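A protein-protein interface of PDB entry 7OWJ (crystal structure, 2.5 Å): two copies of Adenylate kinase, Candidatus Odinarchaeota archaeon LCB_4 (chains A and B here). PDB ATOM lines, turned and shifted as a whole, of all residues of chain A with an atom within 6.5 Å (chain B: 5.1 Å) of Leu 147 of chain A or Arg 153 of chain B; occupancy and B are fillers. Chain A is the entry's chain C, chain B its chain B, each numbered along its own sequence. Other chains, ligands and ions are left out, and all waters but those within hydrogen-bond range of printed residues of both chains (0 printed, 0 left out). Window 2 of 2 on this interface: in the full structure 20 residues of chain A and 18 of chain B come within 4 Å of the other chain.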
ATOM      1  N   PHE A  94      26.518   6.021  25.384  1.00  0.00           N
ATOM      2  CA  PHE A  94      25.097   5.762  25.228  1.00  0.00           C
ATOM      3  C   PHE A  94      24.862   4.420  24.558  1.00  0.00           C
ATOM      4  O   PHE A  94      25.560   4.046  23.614  1.00  0.00           O
ATOM      5  CB  PHE A  94      24.458   6.897  24.433  1.00  0.00           C
ATOM      6  CG  PHE A  94      24.439   8.177  25.183  1.00  0.00           C
ATOM      7  CD1 PHE A  94      23.533   8.392  26.197  1.00  0.00           C
ATOM      8  CD2 PHE A  94      25.366   9.126  24.938  1.00  0.00           C
ATOM      9  CE1 PHE A  94      23.546   9.553  26.922  1.00  0.00           C
ATOM     10  CE2 PHE A  94      25.395  10.265  25.664  1.00  0.00           C
ATOM     11  CZ  PHE A  94      24.492  10.496  26.649  1.00  0.00           C
ATOM     12  N   GLU A 142      22.953  19.574  34.081  1.00  0.00           N
ATOM     13  CA  GLU A 142      21.904  19.850  33.111  1.00  0.00           C
ATOM     14  C   GLU A 142      22.431  19.705  31.686  1.00  0.00           C
ATOM     15  O   GLU A 142      21.672  19.329  30.785  1.00  0.00           O
ATOM     16  CB  GLU A 142      21.241  21.210  33.347  1.00  0.00           C
ATOM     17  CG  GLU A 142      22.033  22.460  33.232  1.00  0.00           C
ATOM     18  CD  GLU A 142      21.173  23.723  33.487  1.00  0.00           C
ATOM     19  OE1 GLU A 142      20.148  23.972  32.791  1.00  0.00           O
ATOM     20  OE2 GLU A 142      21.530  24.459  34.413  1.00  0.00           O
ATOM     21  N   THR A 143      23.729  19.903  31.475  1.00  0.00           N
ATOM     22  CA  THR A 143      24.313  19.639  30.160  1.00  0.00           C
ATOM     23  C   THR A 143      24.291  18.144  29.800  1.00  0.00           C
ATOM     24  O   THR A 143      23.955  17.784  28.660  1.00  0.00           O
ATOM     25  CB  THR A 143      25.730  20.203  30.131  1.00  0.00           C
ATOM     26  OG1 THR A 143      25.630  21.625  29.928  1.00  0.00           O
ATOM     27  CG2 THR A 143      26.586  19.566  29.020  1.00  0.00           C
ATOM     28  N   ASP A 144      24.694  17.267  30.736  1.00  0.00           N
ATOM     29  CA  ASP A 144      24.635  15.829  30.493  1.00  0.00           C
ATOM     30  C   ASP A 144      23.232  15.390  30.106  1.00  0.00           C
ATOM     31  O   ASP A 144      23.037  14.491  29.263  1.00  0.00           O
ATOM     32  CB  ASP A 144      25.044  15.068  31.746  1.00  0.00           C
ATOM     33  CG  ASP A 144      26.513  15.169  32.053  1.00  0.00           C
ATOM     34  OD1 ASP A 144      27.323  15.480  31.138  1.00  0.00           O
ATOM     35  OD2 ASP A 144      26.849  14.891  33.223  1.00  0.00           O
ATOM     36  N   ILE A 145      22.238  16.015  30.727  1.00  0.00           N
ATOM     37  CA  ILE A 145      20.852  15.641  30.525  1.00  0.00           C
ATOM     38  C   ILE A 145      20.349  16.162  29.186  1.00  0.00           C
ATOM     39  O   ILE A 145      19.600  15.475  28.481  1.00  0.00           O
ATOM     40  CB  ILE A 145      20.036  16.176  31.721  1.00  0.00           C
ATOM     41  CG1 ILE A 145      20.408  15.436  33.007  1.00  0.00           C
ATOM     42  CG2 ILE A 145      18.593  16.015  31.475  1.00  0.00           C
ATOM     43  CD1 ILE A 145      19.598  15.846  34.207  1.00  0.00           C
ATOM     44  N   LEU A 146      20.738  17.386  28.829  1.00  0.00           N
ATOM     45  CA  LEU A 146      20.446  17.927  27.503  1.00  0.00           C
ATOM     46  C   LEU A 146      20.967  16.999  26.412  1.00  0.00           C
ATOM     47  O   LEU A 146      20.261  16.669  25.451  1.00  0.00           O
ATOM     48  CB  LEU A 146      21.087  19.293  27.358  1.00  0.00           C
ATOM     49  CG  LEU A 146      20.218  20.559  27.336  1.00  0.00           C
ATOM     50  CD1 LEU A 146      18.875  20.409  26.653  1.00  0.00           C
ATOM     51  CD2 LEU A 146      20.026  20.970  28.722  1.00  0.00           C
ATOM     52  N   LEU A 147      22.206  16.568  26.558  1.00  0.00           N
ATOM     53  CA  LEU A 147      22.813  15.682  25.586  1.00  0.00           C
ATOM     54  C   LEU A 147      22.035  14.386  25.496  1.00  0.00           C
ATOM     55  O   LEU A 147      21.804  13.841  24.398  1.00  0.00           O
ATOM     56  CB  LEU A 147      24.261  15.436  26.004  1.00  0.00           C
ATOM     57  CG  LEU A 147      25.116  14.394  25.300  1.00  0.00           C
ATOM     58  CD1 LEU A 147      25.189  14.719  23.825  1.00  0.00           C
ATOM     59  CD2 LEU A 147      26.464  14.316  25.870  1.00  0.00           C
ATOM     60  N   HIS A 148      21.652  13.853  26.642  1.00  0.00           N
ATOM     61  CA  HIS A 148      20.927  12.596  26.627  1.00  0.00           C
ATOM     62  C   HIS A 148      19.612  12.765  25.866  1.00  0.00           C
ATOM     63  O   HIS A 148      19.291  11.942  25.001  1.00  0.00           O
ATOM     64  CB  HIS A 148      20.733  12.091  28.067  1.00  0.00           C
ATOM     65  CG  HIS A 148      20.313  10.663  28.163  1.00  0.00           C
ATOM     66  ND1 HIS A 148      20.122  10.028  29.367  1.00  0.00           N
ATOM     67  CD2 HIS A 148      20.000   9.756  27.200  1.00  0.00           C
ATOM     68  CE1 HIS A 148      19.716   8.790  29.143  1.00  0.00           C
ATOM     69  NE2 HIS A 148      19.640   8.597  27.835  1.00  0.00           N
ATOM     70  N   GLN A 149      18.875  13.861  26.110  1.00  0.00           N
ATOM     71  CA  GLN A 149      17.570  13.998  25.457  1.00  0.00           C
ATOM     72  C   GLN A 149      17.746  14.203  23.960  1.00  0.00           C
ATOM     73  O   GLN A 149      16.937  13.720  23.156  1.00  0.00           O
ATOM     74  CB  GLN A 149      16.719  15.121  26.091  1.00  0.00           C
ATOM     75  CG  GLN A 149      16.266  14.734  27.510  1.00  0.00           C
ATOM     76  CD  GLN A 149      15.242  15.634  28.133  1.00  0.00           C
ATOM     77  OE1 GLN A 149      14.329  15.171  28.787  1.00  0.00           O
ATOM     78  NE2 GLN A 149      15.403  16.913  27.973  1.00  0.00           N
ATOM     79  N   GLN A 150      18.826  14.838  23.561  1.00  0.00           N
ATOM     80  CA  GLN A 150      19.072  14.983  22.133  1.00  0.00           C
ATOM     81  C   GLN A 150      19.455  13.638  21.500  1.00  0.00           C
ATOM     82  O   GLN A 150      19.059  13.352  20.368  1.00  0.00           O
ATOM     83  CB  GLN A 150      20.130  16.073  21.929  1.00  0.00           C
ATOM     84  CG  GLN A 150      20.302  16.616  20.510  1.00  0.00           C
ATOM     85  CD  GLN A 150      21.627  17.359  20.374  1.00  0.00           C
ATOM     86  OE1 GLN A 150      22.294  17.294  19.346  1.00  0.00           O
ATOM     87  NE2 GLN A 150      22.032  18.037  21.448  1.00  0.00           N
ATOM     88  N   VAL A 151      20.205  12.790  22.210  1.00  0.00           N
ATOM     89  CA  VAL A 151      20.511  11.449  21.695  1.00  0.00           C
ATOM     90  C   VAL A 151      19.230  10.620  21.541  1.00  0.00           C
ATOM     91  O   VAL A 151      19.007   9.976  20.504  1.00  0.00           O
ATOM     92  CB  VAL A 151      21.543  10.752  22.611  1.00  0.00           C
ATOM     93  CG1 VAL A 151      21.586   9.210  22.414  1.00  0.00           C
ATOM     94  CG2 VAL A 151      22.915  11.353  22.405  1.00  0.00           C
ATOM     95  N   ASN A 152      18.361  10.626  22.556  1.00  0.00           N
ATOM     96  CA  ASN A 152      17.110   9.878  22.436  1.00  0.00           C
ATOM     97  C   ASN A 152      16.308  10.352  21.233  1.00  0.00           C
ATOM     98  O   ASN A 152      15.683   9.551  20.501  1.00  0.00           O
ATOM     99  CB  ASN A 152      16.295  10.031  23.707  1.00  0.00           C
ATOM    100  CG  ASN A 152      16.938   9.364  24.863  1.00  0.00           C
ATOM    101  OD1 ASN A 152      17.755   8.441  24.686  1.00  0.00           O
ATOM    102  ND2 ASN A 152      16.589   9.818  26.080  1.00  0.00           N
ATOM    103  N   MET A 154      17.594  11.545  18.553  1.00  0.00           N
ATOM    104  CA  MET A 154      18.216  10.995  17.361  1.00  0.00           C
ATOM    105  C   MET A 154      17.985   9.496  17.217  1.00  0.00           C
ATOM    106  O   MET A 154      17.964   8.994  16.097  1.00  0.00           O
ATOM    107  CB  MET A 154      19.721  11.266  17.354  1.00  0.00           C
ATOM    108  CG  MET A 154      20.113  12.716  17.333  1.00  0.00           C
ATOM    109  SD  MET A 154      21.912  12.927  17.471  1.00  0.00           S
ATOM    110  CE  MET A 154      21.946  14.712  17.235  1.00  0.00           C
ATOM    111  N   LEU B 113      33.378   9.913  19.725  1.00  0.00           N
ATOM    112  CA  LEU B 113      33.465  11.214  19.086  1.00  0.00           C
ATOM    113  C   LEU B 113      34.227  12.167  19.987  1.00  0.00           C
ATOM    114  O   LEU B 113      33.806  12.408  21.131  1.00  0.00           O
ATOM    115  CB  LEU B 113      32.078  11.769  18.796  1.00  0.00           C
ATOM    116  CG  LEU B 113      31.178  11.010  17.827  1.00  0.00           C
ATOM    117  CD1 LEU B 113      30.355  10.046  18.618  1.00  0.00           C
ATOM    118  CD2 LEU B 113      30.237  11.956  17.077  1.00  0.00           C
ATOM    119  N   GLU B 115      34.721  15.909  20.542  1.00  0.00           N
ATOM    120  CA  GLU B 115      34.095  17.194  20.217  1.00  0.00           C
ATOM    121  C   GLU B 115      34.958  18.367  20.696  1.00  0.00           C
ATOM    122  O   GLU B 115      35.256  18.516  21.881  1.00  0.00           O
ATOM    123  CB  GLU B 115      32.678  17.264  20.787  1.00  0.00           C
ATOM    124  CG  GLU B 115      31.879  16.195  20.149  1.00  0.00           C
ATOM    125  CD  GLU B 115      30.390  16.299  20.379  1.00  0.00           C
ATOM    126  OE1 GLU B 115      29.928  17.054  21.275  1.00  0.00           O
ATOM    127  OE2 GLU B 115      29.691  15.597  19.638  1.00  0.00           O
ATOM    128  N   GLN B 149      29.905  19.004  13.609  1.00  0.00           N
ATOM    129  CA  GLN B 149      29.987  18.145  14.795  1.00  0.00           C
ATOM    130  C   GLN B 149      28.619  17.582  15.179  1.00  0.00           C
ATOM    131  O   GLN B 149      28.533  16.432  15.651  1.00  0.00           O
ATOM    132  CB  GLN B 149      30.619  18.864  15.985  1.00  0.00           C
ATOM    133  CG  GLN B 149      32.103  19.176  15.745  1.00  0.00           C
ATOM    134  CD  GLN B 149      32.864  19.561  17.014  1.00  0.00           C
ATOM    135  OE1 GLN B 149      33.990  19.113  17.213  1.00  0.00           O
ATOM    136  NE2 GLN B 149      32.242  20.381  17.880  1.00  0.00           N
ATOM    137  N   GLN B 150      27.545  18.340  14.947  1.00  0.00           N
ATOM    138  CA  GLN B 150      26.210  17.805  15.188  1.00  0.00           C
ATOM    139  C   GLN B 150      25.900  16.692  14.196  1.00  0.00           C
ATOM    140  O   GLN B 150      25.412  15.635  14.587  1.00  0.00           O
ATOM    141  CB  GLN B 150      25.150  18.921  15.118  1.00  0.00           C
ATOM    142  CG  GLN B 150      23.904  18.543  15.957  1.00  0.00           C
ATOM    143  CD  GLN B 150      22.607  19.317  15.616  1.00  0.00           C
ATOM    144  OE1 GLN B 150      22.405  19.821  14.500  1.00  0.00           O
ATOM    145  NE2 GLN B 150      21.717  19.399  16.600  1.00  0.00           N
ATOM    146  N   VAL B 151      26.210  16.906  12.911  1.00  0.00           N
ATOM    147  CA  VAL B 151      25.947  15.902  11.895  1.00  0.00           C
ATOM    148  C   VAL B 151      26.685  14.627  12.258  1.00  0.00           C
ATOM    149  O   VAL B 151      26.150  13.511  12.125  1.00  0.00           O
ATOM    150  CB  VAL B 151      26.363  16.433  10.503  1.00  0.00           C
ATOM    151  CG1 VAL B 151      26.434  15.309   9.482  1.00  0.00           C
ATOM    152  CG2 VAL B 151      25.414  17.524  10.006  1.00  0.00           C
ATOM    153  N   ASN B 152      27.927  14.778  12.730  1.00  0.00           N
ATOM    154  CA  ASN B 152      28.688  13.625  13.186  1.00  0.00           C
ATOM    155  C   ASN B 152      27.938  12.858  14.283  1.00  0.00           C
ATOM    156  O   ASN B 152      27.852  11.613  14.215  1.00  0.00           O
ATOM    157  CB  ASN B 152      30.053  14.094  13.639  1.00  0.00           C
ATOM    158  CG  ASN B 152      30.952  14.396  12.473  1.00  0.00           C
ATOM    159  OD1 ASN B 152      30.648  14.007  11.354  1.00  0.00           O
ATOM    160  ND2 ASN B 152      32.092  15.066  12.727  1.00  0.00           N
ATOM    161  N   ARG B 153      27.343  13.577  15.270  1.00  0.00           N
ATOM    162  CA  ARG B 153      26.519  12.903  16.275  1.00  0.00           C
ATOM    163  C   ARG B 153      25.399  12.085  15.625  1.00  0.00           C
ATOM    164  O   ARG B 153      25.125  10.939  16.024  1.00  0.00           O
ATOM    165  CB  ARG B 153      25.913  13.907  17.242  1.00  0.00           C
ATOM    166  CG  ARG B 153      26.907  14.567  18.217  1.00  0.00           C
ATOM    167  CD  ARG B 153      26.147  15.367  19.257  1.00  0.00           C
ATOM    168  NE  ARG B 153      27.016  16.080  20.183  1.00  0.00           N
ATOM    169  CZ  ARG B 153      26.587  16.820  21.207  1.00  0.00           C
ATOM    170  NH1 ARG B 153      25.290  16.929  21.448  1.00  0.00           N
ATOM    171  NH2 ARG B 153      27.459  17.454  21.995  1.00  0.00           N
ATOM    172  N   MET B 154      24.733  12.663  14.627  1.00  0.00           N
ATOM    173  CA  MET B 154      23.598  11.978  14.017  1.00  0.00           C
ATOM    174  C   MET B 154      24.042  10.718  13.287  1.00  0.00           C
ATOM    175  O   MET B 154      23.392   9.674  13.388  1.00  0.00           O
ATOM    176  CB  MET B 154      22.897  12.928  13.061  1.00  0.00           C
ATOM    177  CG  MET B 154      22.280  14.118  13.781  1.00  0.00           C
ATOM    178  SD  MET B 154      21.594  15.339  12.634  1.00  0.00           S
ATOM    179  CE  MET B 154      20.739  16.378  13.804  1.00  0.00           C
ATOM    180  N   PHE B 155      25.116  10.802  12.525  1.00  0.00           N
ATOM    181  CA  PHE B 155      25.590   9.619  11.845  1.00  0.00           C
ATOM    182  C   PHE B 155      25.848   8.515  12.863  1.00  0.00           C
ATOM    183  O   PHE B 155      25.407   7.367  12.681  1.00  0.00           O
ATOM    184  CB  PHE B 155      26.842   9.946  11.034  1.00  0.00           C
ATOM    185  CG  PHE B 155      26.571  10.430   9.633  1.00  0.00           C
ATOM    186  CD1 PHE B 155      26.178   9.543   8.645  1.00  0.00           C
ATOM    187  CD2 PHE B 155      26.738  11.776   9.283  1.00  0.00           C
ATOM    188  CE1 PHE B 155      25.936  10.001   7.320  1.00  0.00           C
ATOM    189  CE2 PHE B 155      26.494  12.228   7.958  1.00  0.00           C
ATOM    190  CZ  PHE B 155      26.106  11.338   6.990  1.00  0.00           C
ATOM    191  N   ALA B 156      26.527   8.865  13.974  1.00  0.00           N
ATOM    192  CA  ALA B 156      26.918   7.857  14.956  1.00  0.00           C
ATOM    193  C   ALA B 156      25.699   7.211  15.643  1.00  0.00           C
ATOM    194  O   ALA B 156      25.669   5.979  15.825  1.00  0.00           O
ATOM    195  CB  ALA B 156      27.878   8.483  15.968  1.00  0.00           C
ATOM    196  N   VAL B 157      24.674   8.003  16.006  1.00  0.00           N
ATOM    197  CA  VAL B 157      23.491   7.406  16.611  1.00  0.00           C
ATOM    198  C   VAL B 157      22.798   6.513  15.605  1.00  0.00           C
ATOM    199  O   VAL B 157      22.253   5.473  15.961  1.00  0.00           O
ATOM    200  CB  VAL B 157      22.527   8.471  17.183  1.00  0.00           C
ATOM    201  CG1 VAL B 157      21.200   7.822  17.652  1.00  0.00           C
ATOM    202  CG2 VAL B 157      23.182   9.256  18.362  1.00  0.00           C
ATOM    203  N   SER B 158      22.799   6.903  14.331  1.00  0.00           N
ATOM    204  CA  SER B 158      22.217   6.057  13.303  1.00  0.00           C
ATOM    205  C   SER B 158      22.920   4.717  13.256  1.00  0.00           C
ATOM    206  O   SER B 158      22.281   3.671  13.207  1.00  0.00           O
ATOM    207  CB  SER B 158      22.331   6.729  11.945  1.00  0.00           C
ATOM    208  OG  SER B 158      21.279   7.626  11.750  1.00  0.00           O
ATOM    209  N   ILE B 169      30.689  10.313  23.637  1.00  0.00           N
ATOM    210  CA  ILE B 169      30.994  11.685  23.249  1.00  0.00           C
ATOM    211  C   ILE B 169      31.916  12.278  24.295  1.00  0.00           C
ATOM    212  O   ILE B 169      31.489  12.486  25.434  1.00  0.00           O
ATOM    213  CB  ILE B 169      29.724  12.539  23.131  1.00  0.00           C
ATOM    214  CG1 ILE B 169      28.737  11.892  22.158  1.00  0.00           C
ATOM    215  CG2 ILE B 169      30.089  13.934  22.652  1.00  0.00           C
ATOM    216  CD1 ILE B 169      27.443  12.641  22.065  1.00  0.00           C
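The guanidinium group (NH1) of Arg 153 of chain B lies close to the side-chain amide nitrogen (NE2) of Gln 150 of chain A (3.4 Å).
NH2 of Arg 153 of chain B lies within salt-bridge range of OE1 of Glu 115 of chain B.
OG of Ser 158 of chain B is in hydrogen-bond range of O of Met 154 of chain B (3.4 Å).
CD1 of Leu 147 of chain A touches NH1 of Arg 153 of chain B (3.2 Å).
Ile 169 of chain B touches Leu 147 of chain A.
Gln 150 of chain B touches Gln 150 of chain A.
Met 154 of chain B touches Met 154 of chain A (CG to CE, 3.5 Å).
Val 157 of chain B touches Met 154 of chain A.
Of chain A, only Leu 147 (3.2 Å) and Gln 150 (3.4 Å) come within 4 Å of Arg 153 of chain B.
Printed residues of chain A within 4 Å of Val 157 of chain B: Met 154.
Printed residues of chain B within 4 Å of Gln 150 of chain A: Gln 150 and Arg 153.
The nearest printed residue of chain B that does not touch Leu 147 of chain A is Glu 115 of chain B (5.9 Å).
Printed residues of chain B that touch a printed residue of chain A: Gln 150, Arg 153, Met 154, Val 157 and Ile 169.
Hydrophobic or aromatic side chains of chain B within 4 Å of the printed part of chain A: Met 154, Val 157 and Ile 169.
Of the 13 printed residues of chain A, 3 touch a printed residue of chain B.
Hydrophobic or aromatic side chains of chain A that line the printed part of chain B: Leu 147 and Met 154.
Among the printed residues, 6 pairs touch across the chains.
Gln 150 of chain A touches its own counterpart, Gln 150 of chain B.
Met 154 of chain A touches its own counterpart, Met 154 of chain B.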
